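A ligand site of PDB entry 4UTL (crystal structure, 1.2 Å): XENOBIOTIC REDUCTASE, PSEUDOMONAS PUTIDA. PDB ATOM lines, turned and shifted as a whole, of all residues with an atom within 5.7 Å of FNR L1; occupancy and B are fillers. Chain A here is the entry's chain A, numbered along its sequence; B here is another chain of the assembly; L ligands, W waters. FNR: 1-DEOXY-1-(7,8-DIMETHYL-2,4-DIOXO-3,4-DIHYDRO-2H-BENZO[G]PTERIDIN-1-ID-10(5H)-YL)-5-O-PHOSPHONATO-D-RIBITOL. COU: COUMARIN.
An oxygen (O3P) of FNR L1 is in hydrogen-bond range of the backbone NH of Gly 327 (2.7 Å).
The guanidinium group (NE) of Arg 328 is in salt-bridge range of an oxygen (O1P) of FNR L1, 2.8 Å away.
A ring nitrogen (NE2) of His 180 is in hydrogen-bond range of an oxygen (O1) of COU L2, 3.0 Å away.
An oxygen (O4) of FNR L1 sits at hydrogen-bond distance from the side-chain sulfur of Cys 27 (3.3 Å).
The backbone NH of Gly 305 sits at hydrogen-bond distance from an oxygen (O2P) of FNR L1 (2.9 Å).
The guanidinium group (NH2) of Arg 328 lies close to an oxygen (O2) of COU L3, 3.1 Å away.
OE1 of Gln 101 sits at hydrogen-bond distance from N3 of FNR L1 (2.9 Å).
An oxygen (O4) of FNR L1 sits close to the backbone NH of Cys 27 (3.4 Å).
N of Arg 328 sits at hydrogen-bond distance from O1P of FNR L1, 2.9 Å away.
A ring nitrogen (ND1) of His 183 lies close to an oxygen (O2) of FNR L1.
NH1 of Arg 233 lies within hydrogen-bond range of O2 of FNR L1, at 2.8 Å.
The backbone NH (N) of Ala 59 sits at hydrogen-bond distance from an oxygen (O4) of FNR L1.
A ring nitrogen (NE2) of His 180 sits at hydrogen-bond distance from an oxygen (O2) of FNR L1, 3.3 Å away.
O2' of FNR L1 lies within hydrogen-bond range of O of Pro 25 (2.9 Å).
The backbone NH (N) of Trp 304 is in hydrogen-bond range of an oxygen (O5') of FNR L1 (3.1 Å).
ND1 of His 183 sits at hydrogen-bond distance from O1 of COU L2.
Water W1 lies within hydrogen-bond range of an oxygen (O3P) of FNR L1 (2.7 Å), the backbone carbonyl oxygen (O) of Ser 325 (2.8 Å), the backbone NH (N) of Phe 306 (2.9 Å) and the backbone NH (N) of Trp 304 (3.4 Å).
Water W3 lies within hydrogen-bond range of an oxygen (O3P) of FNR L1, the backbone NH (N) of Ala 329 and the backbone NH (N) of Arg 328.
Merely in contact with FNR L1: Pro 24 (3.4 Å), Met 26 (3.4 Å), Glu 58 (3.96 Å), Ala 303 (3.5 Å), Val 326 (3.7 Å), Leu 331 (3.9 Å) and Trp 360 of chain B (3.2 Å).
Hydrophobic or aromatic side chains within 4 Å of FNR L1: Pro 24, Pro 25, Met 26, Ala 59, His 180, His 183, Ala 303, Trp 304, Leu 331 and Trp 360 of chain B.
Within 4 Å of FNR L1: Pro 24, Pro 25, Met 26, Cys 27, Glu 58, Ala 59, Gln 101, His 180, His 183, Arg 233, Ala 303, Trp 304, Gly 305, Val 326, Gly 327, Arg 328, Leu 331 and Trp 360 of chain B.
O1 of COU L2 sits close to N3 of FNR L1 (3.3 Å).
OE1 of Glu 58 lies within hydrogen-bond range of N of Gln 28 (3.0 Å).
The side-chain amide nitrogen of Gln 101 sits at hydrogen-bond distance from the side-chain carboxylate of Glu 178, at 2.7 Å.
O of Met 26 sits at hydrogen-bond distance from NE2 of Gln 28, at 3.0 Å.
NE2 of His 183 sits at hydrogen-bond distance from OG of Ser 268.
The backbone NH (N) of Ala 59 sits close to the side-chain amide oxygen (OE1) of Gln 101 (3.4 Å).
The indole nitrogen (NE1) of Trp 304 is in hydrogen-bond range of the side-chain hydroxyl (OG) of Ser 268 (2.9 Å).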
ATOM      1  N   PRO A  24      -8.550  -7.136 -18.787  1.00  0.00           N
ATOM      2  CA  PRO A  24      -8.538  -7.910 -20.033  1.00  0.00           C
ATOM      3  C   PRO A  24      -7.397  -8.915 -20.003  1.00  0.00           C
ATOM      4  O   PRO A  24      -6.461  -8.760 -19.190  1.00  0.00           O
ATOM      5  CB  PRO A  24      -8.326  -6.843 -21.094  1.00  0.00           C
ATOM      6  CG  PRO A  24      -7.447  -5.846 -20.387  1.00  0.00           C
ATOM      7  CD  PRO A  24      -7.981  -5.797 -18.987  1.00  0.00           C
ATOM      8  N   PRO A  25      -7.417  -9.900 -20.890  1.00  0.00           N
ATOM      9  CA  PRO A  25      -6.323 -10.862 -20.963  1.00  0.00           C
ATOM     10  C   PRO A  25      -4.993 -10.149 -21.232  1.00  0.00           C
ATOM     11  O   PRO A  25      -4.910  -9.305 -22.118  1.00  0.00           O
ATOM     12  CB  PRO A  25      -6.745 -11.781 -22.127  1.00  0.00           C
ATOM     13  CG  PRO A  25      -7.716 -10.936 -22.946  1.00  0.00           C
ATOM     14  CD  PRO A  25      -8.436 -10.115 -21.929  1.00  0.00           C
ATOM     15  N   MET A  26      -3.973 -10.502 -20.461  1.00  0.00           N
ATOM     16  CA  MET A  26      -2.631  -9.944 -20.628  1.00  0.00           C
ATOM     17  C   MET A  26      -1.578 -11.030 -20.434  1.00  0.00           C
ATOM     18  O   MET A  26      -1.252 -11.452 -19.322  1.00  0.00           O
ATOM     19  CB  MET A  26      -2.341  -8.792 -19.678  1.00  0.00           C
ATOM     20  CG  MET A  26      -3.122  -7.528 -20.004  1.00  0.00           C
ATOM     21  SD  MET A  26      -2.733  -6.139 -18.932  1.00  0.00           S
ATOM     22  CE  MET A  26      -3.584  -6.650 -17.432  1.00  0.00           C
ATOM     23  N   CYS A  27      -1.065 -11.524 -21.548  1.00  0.00           N
ATOM     24  CA  CYS A  27       0.055 -12.470 -21.593  1.00  0.00           C
ATOM     25  C   CYS A  27       1.176 -12.077 -20.682  1.00  0.00           C
ATOM     26  O   CYS A  27       1.604 -10.905 -20.664  1.00  0.00           O
ATOM     27  CB  CYS A  27       0.595 -12.574 -23.027  1.00  0.00           C
ATOM     28  SG  CYS A  27      -0.393 -13.568 -24.142  1.00  0.00           S
ATOM     29  N   GLN A  28       1.677 -13.051 -19.943  1.00  0.00           N
ATOM     30  CA  GLN A  28       2.760 -12.867 -18.996  1.00  0.00           C
ATOM     31  C   GLN A  28       4.074 -13.494 -19.485  1.00  0.00           C
ATOM     32  O   GLN A  28       5.133 -13.164 -18.969  1.00  0.00           O
ATOM     33  CB  GLN A  28       2.384 -13.475 -17.648  1.00  0.00           C
ATOM     34  CG  GLN A  28       1.180 -12.797 -16.996  1.00  0.00           C
ATOM     35  CD  GLN A  28       1.477 -11.373 -16.665  1.00  0.00           C
ATOM     36  OE1 GLN A  28       2.220 -11.079 -15.733  1.00  0.00           O
ATOM     37  NE2 GLN A  28       0.903 -10.450 -17.451  1.00  0.00           N
ATOM     38  N   TYR A  29       4.003 -14.439 -20.416  1.00  0.00           N
ATOM     39  CA  TYR A  29       5.194 -15.051 -21.029  1.00  0.00           C
ATOM     40  C   TYR A  29       6.042 -15.807 -19.979  1.00  0.00           C
ATOM     41  O   TYR A  29       7.264 -15.935 -20.145  1.00  0.00           O
ATOM     42  CB  TYR A  29       6.042 -14.049 -21.821  1.00  0.00           C
ATOM     43  CG  TYR A  29       5.220 -13.206 -22.774  1.00  0.00           C
ATOM     44  CD1 TYR A  29       4.937 -13.649 -24.064  1.00  0.00           C
ATOM     45  CD2 TYR A  29       4.675 -11.992 -22.377  1.00  0.00           C
ATOM     46  CE1 TYR A  29       4.179 -12.890 -24.923  1.00  0.00           C
ATOM     47  CE2 TYR A  29       3.911 -11.234 -23.243  1.00  0.00           C
ATOM     48  CZ  TYR A  29       3.682 -11.662 -24.518  1.00  0.00           C
ATOM     49  OH  TYR A  29       2.929 -10.879 -25.358  1.00  0.00           O
ATOM     50  N   GLU A  58      -5.001 -14.397 -19.440  1.00  0.00           N
ATOM     51  CA  GLU A  58      -4.288 -14.252 -20.700  1.00  0.00           C
ATOM     52  C   GLU A  58      -4.595 -15.297 -21.739  1.00  0.00           C
ATOM     53  O   GLU A  58      -4.979 -16.414 -21.411  1.00  0.00           O
ATOM     54  CB  GLU A  58      -2.787 -14.308 -20.424  1.00  0.00           C
ATOM     55  CG  GLU A  58      -2.281 -15.673 -19.856  1.00  0.00           C
ATOM     56  CD  GLU A  58      -0.902 -15.532 -19.237  1.00  0.00           C
ATOM     57  OE1 GLU A  58       0.125 -15.613 -19.959  1.00  0.00           O
ATOM     58  OE2 GLU A  58      -0.829 -15.293 -18.015  1.00  0.00           O
ATOM     59  N   ALA A  59      -4.335 -14.936 -23.001  1.00  0.00           N
ATOM     60  CA  ALA A  59      -4.438 -15.873 -24.136  1.00  0.00           C
ATOM     61  C   ALA A  59      -3.796 -17.201 -23.781  1.00  0.00           C
ATOM     62  O   ALA A  59      -2.589 -17.272 -23.563  1.00  0.00           O
ATOM     63  CB  ALA A  59      -3.749 -15.276 -25.343  1.00  0.00           C
ATOM     64  N   GLN A 101      -9.320 -16.437 -21.680  1.00  0.00           N
ATOM     65  CA  GLN A 101      -9.278 -16.298 -23.123  1.00  0.00           C
ATOM     66  C   GLN A 101      -8.575 -17.495 -23.735  1.00  0.00           C
ATOM     67  O   GLN A 101      -7.419 -17.745 -23.408  1.00  0.00           O
ATOM     68  CB  GLN A 101      -8.562 -14.990 -23.516  1.00  0.00           C
ATOM     69  CG  GLN A 101      -8.627 -14.711 -25.000  1.00  0.00           C
ATOM     70  CD  GLN A 101      -7.759 -13.546 -25.393  1.00  0.00           C
ATOM     71  OE1 GLN A 101      -6.560 -13.608 -25.183  1.00  0.00           O
ATOM     72  NE2 GLN A 101      -8.336 -12.510 -25.966  1.00  0.00           N
ATOM     73  N   GLU A 178     -13.709 -16.383 -23.230  1.00  0.00           N
ATOM     74  CA  GLU A 178     -13.534 -15.468 -24.350  1.00  0.00           C
ATOM     75  C   GLU A 178     -12.787 -16.189 -25.452  1.00  0.00           C
ATOM     76  O   GLU A 178     -11.640 -16.641 -25.253  1.00  0.00           O
ATOM     77  CB  GLU A 178     -12.748 -14.216 -23.936  1.00  0.00           C
ATOM     78  CG  GLU A 178     -12.655 -13.160 -25.024  1.00  0.00           C
ATOM     79  CD  GLU A 178     -11.893 -11.912 -24.561  1.00  0.00           C
ATOM     80  OE1 GLU A 178     -12.444 -11.134 -23.757  1.00  0.00           O
ATOM     81  OE2 GLU A 178     -10.748 -11.720 -24.994  1.00  0.00           O
ATOM     82  N   HIS A 180     -10.594 -16.039 -28.638  1.00  0.00           N
ATOM     83  CA  HIS A 180      -9.681 -15.045 -29.174  1.00  0.00           C
ATOM     84  C   HIS A 180      -9.699 -15.011 -30.690  1.00  0.00           C
ATOM     85  O   HIS A 180      -8.926 -15.723 -31.341  1.00  0.00           O
ATOM     86  CB  HIS A 180      -8.249 -15.285 -28.688  1.00  0.00           C
ATOM     87  CG  HIS A 180      -7.374 -14.095 -28.847  1.00  0.00           C
ATOM     88  ND1 HIS A 180      -7.757 -12.980 -29.571  1.00  0.00           N
ATOM     89  CD2 HIS A 180      -6.164 -13.804 -28.310  1.00  0.00           C
ATOM     90  CE1 HIS A 180      -6.815 -12.050 -29.466  1.00  0.00           C
ATOM     91  NE2 HIS A 180      -5.835 -12.529 -28.714  1.00  0.00           N
ATOM     92  N   HIS A 183      -6.593  -9.698 -33.236  1.00  0.00           N
ATOM     93  CA  HIS A 183      -5.171  -9.404 -33.095  1.00  0.00           C
ATOM     94  C   HIS A 183      -4.293 -10.163 -34.090  1.00  0.00           C
ATOM     95  O   HIS A 183      -3.100 -10.347 -33.878  1.00  0.00           O
ATOM     96  CB  HIS A 183      -4.686  -9.566 -31.660  1.00  0.00           C
ATOM     97  CG  HIS A 183      -5.450  -8.704 -30.694  1.00  0.00           C
ATOM     98  ND1 HIS A 183      -5.319  -8.825 -29.329  1.00  0.00           N
ATOM     99  CD2 HIS A 183      -6.334  -7.701 -30.901  1.00  0.00           C
ATOM    100  CE1 HIS A 183      -6.114  -7.949 -28.732  1.00  0.00           C
ATOM    101  NE2 HIS A 183      -6.743  -7.255 -29.667  1.00  0.00           N
ATOM    102  N   ARG A 233     -13.378 -11.936 -28.462  1.00  0.00           N
ATOM    103  CA  ARG A 233     -12.669 -10.730 -28.856  1.00  0.00           C
ATOM    104  C   ARG A 233     -12.481 -10.741 -30.346  1.00  0.00           C
ATOM    105  O   ARG A 233     -12.089 -11.757 -30.918  1.00  0.00           O
ATOM    106  CB  ARG A 233     -11.330 -10.623 -28.112  1.00  0.00           C
ATOM    107  CG  ARG A 233     -10.758  -9.210 -28.164  1.00  0.00           C
ATOM    108  CD  ARG A 233      -9.614  -9.000 -27.196  1.00  0.00           C
ATOM    109  NE  ARG A 233      -9.575  -7.617 -26.775  1.00  0.00           N
ATOM    110  CZ  ARG A 233      -8.686  -7.095 -25.925  1.00  0.00           C
ATOM    111  NH1 ARG A 233      -7.654  -7.803 -25.502  1.00  0.00           N
ATOM    112  NH2 ARG A 233      -8.843  -5.821 -25.549  1.00  0.00           N
ATOM    113  N   SER A 268     -12.098  -4.886 -30.620  1.00  0.00           N
ATOM    114  CA  SER A 268     -10.703  -4.539 -30.725  1.00  0.00           C
ATOM    115  C   SER A 268     -10.322  -4.165 -32.153  1.00  0.00           C
ATOM    116  O   SER A 268     -11.200  -3.951 -33.025  1.00  0.00           O
ATOM    117  CB  SER A 268      -9.867  -5.698 -30.196  1.00  0.00           C
ATOM    118  OG  SER A 268      -8.563  -5.271 -29.867  1.00  0.00           O
ATOM    119  N   ALA A 303     -10.916  -1.590 -24.857  1.00  0.00           N
ATOM    120  CA  ALA A 303      -9.703  -1.277 -24.108  1.00  0.00           C
ATOM    121  C   ALA A 303      -8.915  -0.288 -24.966  1.00  0.00           C
ATOM    122  O   ALA A 303      -9.496   0.360 -25.826  1.00  0.00           O
ATOM    123  CB  ALA A 303      -8.889  -2.560 -23.849  1.00  0.00           C
ATOM    124  N   TRP A 304      -7.609  -0.217 -24.784  1.00  0.00           N
ATOM    125  CA  TRP A 304      -6.704   0.580 -25.614  1.00  0.00           C
ATOM    126  C   TRP A 304      -6.841   2.062 -25.339  1.00  0.00           C
ATOM    127  O   TRP A 304      -7.067   2.874 -26.252  1.00  0.00           O
ATOM    128  CB  TRP A 304      -6.881   0.303 -27.115  1.00  0.00           C
ATOM    129  CG  TRP A 304      -6.854  -1.149 -27.487  1.00  0.00           C
ATOM    130  CD1 TRP A 304      -7.930  -1.928 -27.816  1.00  0.00           C
ATOM    131  CD2 TRP A 304      -5.701  -1.993 -27.609  1.00  0.00           C
ATOM    132  NE1 TRP A 304      -7.521  -3.189 -28.136  1.00  0.00           N
ATOM    133  CE2 TRP A 304      -6.159  -3.258 -28.030  1.00  0.00           C
ATOM    134  CE3 TRP A 304      -4.325  -1.790 -27.450  1.00  0.00           C
ATOM    135  CZ2 TRP A 304      -5.292  -4.327 -28.258  1.00  0.00           C
ATOM    136  CZ3 TRP A 304      -3.465  -2.849 -27.673  1.00  0.00           C
ATOM    137  CH2 TRP A 304      -3.954  -4.101 -28.068  1.00  0.00           C
ATOM    138  N   GLY A 305      -6.687   2.435 -24.067  1.00  0.00           N
ATOM    139  CA  GLY A 305      -6.712   3.832 -23.659  1.00  0.00           C
ATOM    140  C   GLY A 305      -7.890   4.268 -22.805  1.00  0.00           C
ATOM    141  O   GLY A 305      -8.119   5.472 -22.731  1.00  0.00           O
ATOM    142  N   PHE A 306      -8.602   3.356 -22.140  1.00  0.00           N
ATOM    143  CA  PHE A 306      -9.654   3.762 -21.203  1.00  0.00           C
ATOM    144  C   PHE A 306      -9.183   3.814 -19.758  1.00  0.00           C
ATOM    145  O   PHE A 306      -9.981   4.055 -18.867  1.00  0.00           O
ATOM    146  CB  PHE A 306     -10.876   2.861 -21.279  1.00  0.00           C
ATOM    147  CG  PHE A 306     -11.642   2.959 -22.556  1.00  0.00           C
ATOM    148  CD1 PHE A 306     -12.598   3.961 -22.739  1.00  0.00           C
ATOM    149  CD2 PHE A 306     -11.455   2.048 -23.563  1.00  0.00           C
ATOM    150  CE1 PHE A 306     -13.323   4.015 -23.921  1.00  0.00           C
ATOM    151  CE2 PHE A 306     -12.145   2.088 -24.720  1.00  0.00           C
ATOM    152  CZ  PHE A 306     -13.077   3.059 -24.918  1.00  0.00           C
ATOM    153  N   GLY A 307      -7.890   3.616 -19.537  1.00  0.00           N
ATOM    154  CA  GLY A 307      -7.366   3.463 -18.195  1.00  0.00           C
ATOM    155  C   GLY A 307      -7.140   4.689 -17.338  1.00  0.00           C
ATOM    156  O   GLY A 307      -6.095   4.832 -16.717  1.00  0.00           O
ATOM    157  N   SER A 325     -12.517  -2.325 -19.989  1.00  0.00           N
ATOM    158  CA  SER A 325     -11.320  -3.117 -19.780  1.00  0.00           C
ATOM    159  C   SER A 325     -10.126  -2.208 -19.571  1.00  0.00           C
ATOM    160  O   SER A 325      -9.879  -1.325 -20.395  1.00  0.00           O
ATOM    161  CB  SER A 325     -11.108  -4.072 -20.951  1.00  0.00           C
ATOM    162  OG  SER A 325     -12.178  -4.998 -21.050  1.00  0.00           O
ATOM    163  N   VAL A 326      -9.398  -2.459 -18.488  1.00  0.00           N
ATOM    164  CA  VAL A 326      -8.265  -1.643 -18.069  1.00  0.00           C
ATOM    165  C   VAL A 326      -7.072  -2.588 -17.866  1.00  0.00           C
ATOM    166  O   VAL A 326      -7.027  -3.375 -16.917  1.00  0.00           O
ATOM    167  CB  VAL A 326      -8.606  -0.879 -16.770  1.00  0.00           C
ATOM    168  CG1 VAL A 326      -7.396  -0.083 -16.307  1.00  0.00           C
ATOM    169  CG2 VAL A 326      -9.767   0.042 -17.010  1.00  0.00           C
ATOM    170  N   GLY A 327      -6.103  -2.498 -18.774  1.00  0.00           N
ATOM    171  CA  GLY A 327      -4.972  -3.394 -18.825  1.00  0.00           C
ATOM    172  C   GLY A 327      -3.695  -2.891 -18.186  1.00  0.00           C
ATOM    173  O   GLY A 327      -3.390  -3.236 -17.029  1.00  0.00           O
ATOM    174  N   ARG A 328      -2.940  -2.055 -18.902  1.00  0.00           N
ATOM    175  CA  ARG A 328      -1.638  -1.621 -18.394  1.00  0.00           C
ATOM    176  C   ARG A 328      -1.707  -0.934 -17.039  1.00  0.00           C
ATOM    177  O   ARG A 328      -0.788  -1.083 -16.218  1.00  0.00           O
ATOM    178  CB  ARG A 328      -0.957  -0.722 -19.410  1.00  0.00           C
ATOM    179  CG  ARG A 328      -0.415  -1.481 -20.619  1.00  0.00           C
ATOM    180  CD  ARG A 328       0.001  -0.563 -21.739  1.00  0.00           C
ATOM    181  NE  ARG A 328      -1.175   0.134 -22.248  1.00  0.00           N
ATOM    182  CZ  ARG A 328      -1.157   1.322 -22.844  1.00  0.00           C
ATOM    183  NH1 ARG A 328      -0.007   1.936 -23.096  1.00  0.00           N
ATOM    184  NH2 ARG A 328      -2.300   1.865 -23.243  1.00  0.00           N
ATOM    185  N   ALA A 329      -2.762  -0.183 -16.768  1.00  0.00           N
ATOM    186  CA  ALA A 329      -2.877   0.483 -15.463  1.00  0.00           C
ATOM    187  C   ALA A 329      -2.870  -0.528 -14.311  1.00  0.00           C
ATOM    188  O   ALA A 329      -2.444  -0.177 -13.213  1.00  0.00           O
ATOM    189  CB  ALA A 329      -4.100   1.372 -15.423  1.00  0.00           C
ATOM    190  N   LEU A 331      -1.118  -3.424 -14.425  1.00  0.00           N
ATOM    191  CA  LEU A 331       0.265  -3.860 -14.278  1.00  0.00           C
ATOM    192  C   LEU A 331       1.016  -2.847 -13.416  1.00  0.00           C
ATOM    193  O   LEU A 331       1.812  -3.226 -12.533  1.00  0.00           O
ATOM    194  CB  LEU A 331       0.947  -4.027 -15.638  1.00  0.00           C
ATOM    195  CG  LEU A 331       0.240  -4.955 -16.624  1.00  0.00           C
ATOM    196  CD1 LEU A 331       1.061  -5.013 -17.927  1.00  0.00           C
ATOM    197  CD2 LEU A 331       0.003  -6.342 -16.062  1.00  0.00           C
ATOM    198  N   PRO B 356       7.614  -9.013 -17.020  1.00  0.00           N
ATOM    199  CA  PRO B 356       6.262  -9.071 -17.572  1.00  0.00           C
ATOM    200  C   PRO B 356       5.440  -7.852 -17.306  1.00  0.00           C
ATOM    201  O   PRO B 356       4.396  -7.680 -17.923  1.00  0.00           O
ATOM    202  CB  PRO B 356       5.663 -10.321 -16.901  1.00  0.00           C
ATOM    203  CG  PRO B 356       6.822 -11.123 -16.477  1.00  0.00           C
ATOM    204  CD  PRO B 356       7.869 -10.147 -16.108  1.00  0.00           C
ATOM    205  N   TRP B 360       6.203  -3.275 -20.556  1.00  0.00           N
ATOM    206  CA  TRP B 360       5.033  -2.558 -21.074  1.00  0.00           C
ATOM    207  C   TRP B 360       4.852  -1.177 -20.508  1.00  0.00           C
ATOM    208  O   TRP B 360       4.034  -0.426 -20.997  1.00  0.00           O
ATOM    209  CB  TRP B 360       3.781  -3.388 -20.797  1.00  0.00           C
ATOM    210  CG  TRP B 360       3.958  -4.767 -21.278  1.00  0.00           C
ATOM    211  CD1 TRP B 360       4.219  -5.884 -20.525  1.00  0.00           C
ATOM    212  CD2 TRP B 360       4.010  -5.183 -22.646  1.00  0.00           C
ATOM    213  NE1 TRP B 360       4.393  -6.961 -21.352  1.00  0.00           N
ATOM    214  CE2 TRP B 360       4.242  -6.569 -22.657  1.00  0.00           C
ATOM    215  CE3 TRP B 360       3.845  -4.526 -23.869  1.00  0.00           C
ATOM    216  CZ2 TRP B 360       4.326  -7.297 -23.826  1.00  0.00           C
ATOM    217  CZ3 TRP B 360       3.941  -5.231 -25.027  1.00  0.00           C
ATOM    218  CH2 TRP B 360       4.171  -6.623 -25.009  1.00  0.00           C
HETATM  219  C9A FNR L   1      -2.076  -7.530 -23.908  1.00  0.00           C
HETATM  220  N10 FNR L   1      -3.215  -7.598 -24.731  1.00  0.00           N
HETATM  221  CAA FNR L   1      -3.802  -8.873 -24.979  1.00  0.00           C
HETATM  222  N1  FNR L   1      -4.934  -8.964 -25.627  1.00  0.00           N
HETATM  223  C2  FNR L   1      -5.468 -10.134 -25.795  1.00  0.00           C
HETATM  224  O2  FNR L   1      -6.557 -10.250 -26.422  1.00  0.00           O
HETATM  225  N3  FNR L   1      -4.893 -11.250 -25.217  1.00  0.00           N
HETATM  226  C4  FNR L   1      -3.785 -11.230 -24.560  1.00  0.00           C
HETATM  227  O4  FNR L   1      -3.368 -12.222 -23.973  1.00  0.00           O
HETATM  228  C4A FNR L   1      -3.077 -10.011 -24.532  1.00  0.00           C
HETATM  229  N5  FNR L   1      -1.821  -9.924 -23.955  1.00  0.00           N
HETATM  230  C5A FNR L   1      -1.394  -8.686 -23.568  1.00  0.00           C
HETATM  231  C6  FNR L   1      -0.216  -8.608 -22.686  1.00  0.00           C
HETATM  232  C7  FNR L   1       0.180  -7.341 -22.155  1.00  0.00           C
HETATM  233  C7M FNR L   1       1.248  -7.335 -21.104  1.00  0.00           C
HETATM  234  C8  FNR L   1      -0.513  -6.202 -22.535  1.00  0.00           C
HETATM  235  C8M FNR L   1      -0.077  -4.885 -22.023  1.00  0.00           C
HETATM  236  C9  FNR L   1      -1.580  -6.251 -23.401  1.00  0.00           C
HETATM  237  C1' FNR L   1      -4.040  -6.411 -24.948  1.00  0.00           C
HETATM  238  C2' FNR L   1      -4.770  -5.950 -23.699  1.00  0.00           C
HETATM  239  O2' FNR L   1      -5.834  -6.864 -23.384  1.00  0.00           O
HETATM  240  C3' FNR L   1      -5.385  -4.557 -23.833  1.00  0.00           C
HETATM  241  O3' FNR L   1      -6.251  -4.545 -24.975  1.00  0.00           O
HETATM  242  C4' FNR L   1      -4.347  -3.451 -24.013  1.00  0.00           C
HETATM  243  O4' FNR L   1      -3.382  -3.528 -22.935  1.00  0.00           O
HETATM  244  C5' FNR L   1      -4.991  -2.058 -24.135  1.00  0.00           C
HETATM  245  O5' FNR L   1      -5.657  -1.706 -22.895  1.00  0.00           O
HETATM  246  P   FNR L   1      -4.933  -0.614 -21.903  1.00  0.00           P
HETATM  247  O1P FNR L   1      -3.548  -1.225 -21.573  1.00  0.00           O
HETATM  248  O2P FNR L   1      -4.817   0.699 -22.641  1.00  0.00           O
HETATM  249  O3P FNR L   1      -5.890  -0.567 -20.692  1.00  0.00           O
HETATM  250  C1  COU L   2      -2.488 -10.296 -27.720  1.00  0.00           C
HETATM  251  C2  COU L   2      -1.421 -11.070 -27.206  1.00  0.00           C
HETATM  252  C3  COU L   2      -0.281 -10.435 -26.717  1.00  0.00           C
HETATM  253  C4  COU L   2      -0.227  -9.039 -26.747  1.00  0.00           C
HETATM  254  C5  COU L   2       0.867  -8.318 -26.273  1.00  0.00           C
HETATM  255  C6  COU L   2       0.865  -6.927 -26.320  1.00  0.00           C
HETATM  256  C7  COU L   2      -0.218  -6.235 -26.830  1.00  0.00           C
HETATM  257  C8  COU L   2      -1.299  -6.935 -27.307  1.00  0.00           C
HETATM  258  C9  COU L   2      -1.291  -8.314 -27.254  1.00  0.00           C
HETATM  259  O1  COU L   2      -3.510 -10.723 -28.155  1.00  0.00           O
HETATM  260  O2  COU L   2      -2.390  -8.936 -27.743  1.00  0.00           O
HETATM  261  C1  COU L   3      -2.361   1.140 -26.218  1.00  0.00           C
HETATM  262  C2  COU L   3      -1.271   1.820 -26.755  1.00  0.00           C
HETATM  263  C3  COU L   3      -0.006   1.225 -26.742  1.00  0.00           C
HETATM  264  C4  COU L   3       0.148  -0.052 -26.201  1.00  0.00           C
HETATM  265  C5  COU L   3       1.393  -0.667 -26.180  1.00  0.00           C
HETATM  266  C6  COU L   3       1.525  -1.935 -25.635  1.00  0.00           C
HETATM  267  C7  COU L   3       0.427  -2.596 -25.108  1.00  0.00           C
HETATM  268  C8  COU L   3      -0.818  -1.971 -25.131  1.00  0.00           C
HETATM  269  C9  COU L   3      -0.957  -0.703 -25.670  1.00  0.00           C
HETATM  270  O1  COU L   3      -3.507   1.634 -26.209  1.00  0.00           O
HETATM  271  O2  COU L   3      -2.186  -0.107 -25.688  1.00  0.00           O
HETATM  272  O   HOH W   1      -8.202   0.599 -21.495  1.00  0.00           O
HETATM  273  O   HOH W   2      -5.445   2.882 -20.959  1.00  0.00           O
HETATM  274  O   HOH W   3      -4.687   0.847 -18.617  1.00  0.00           O
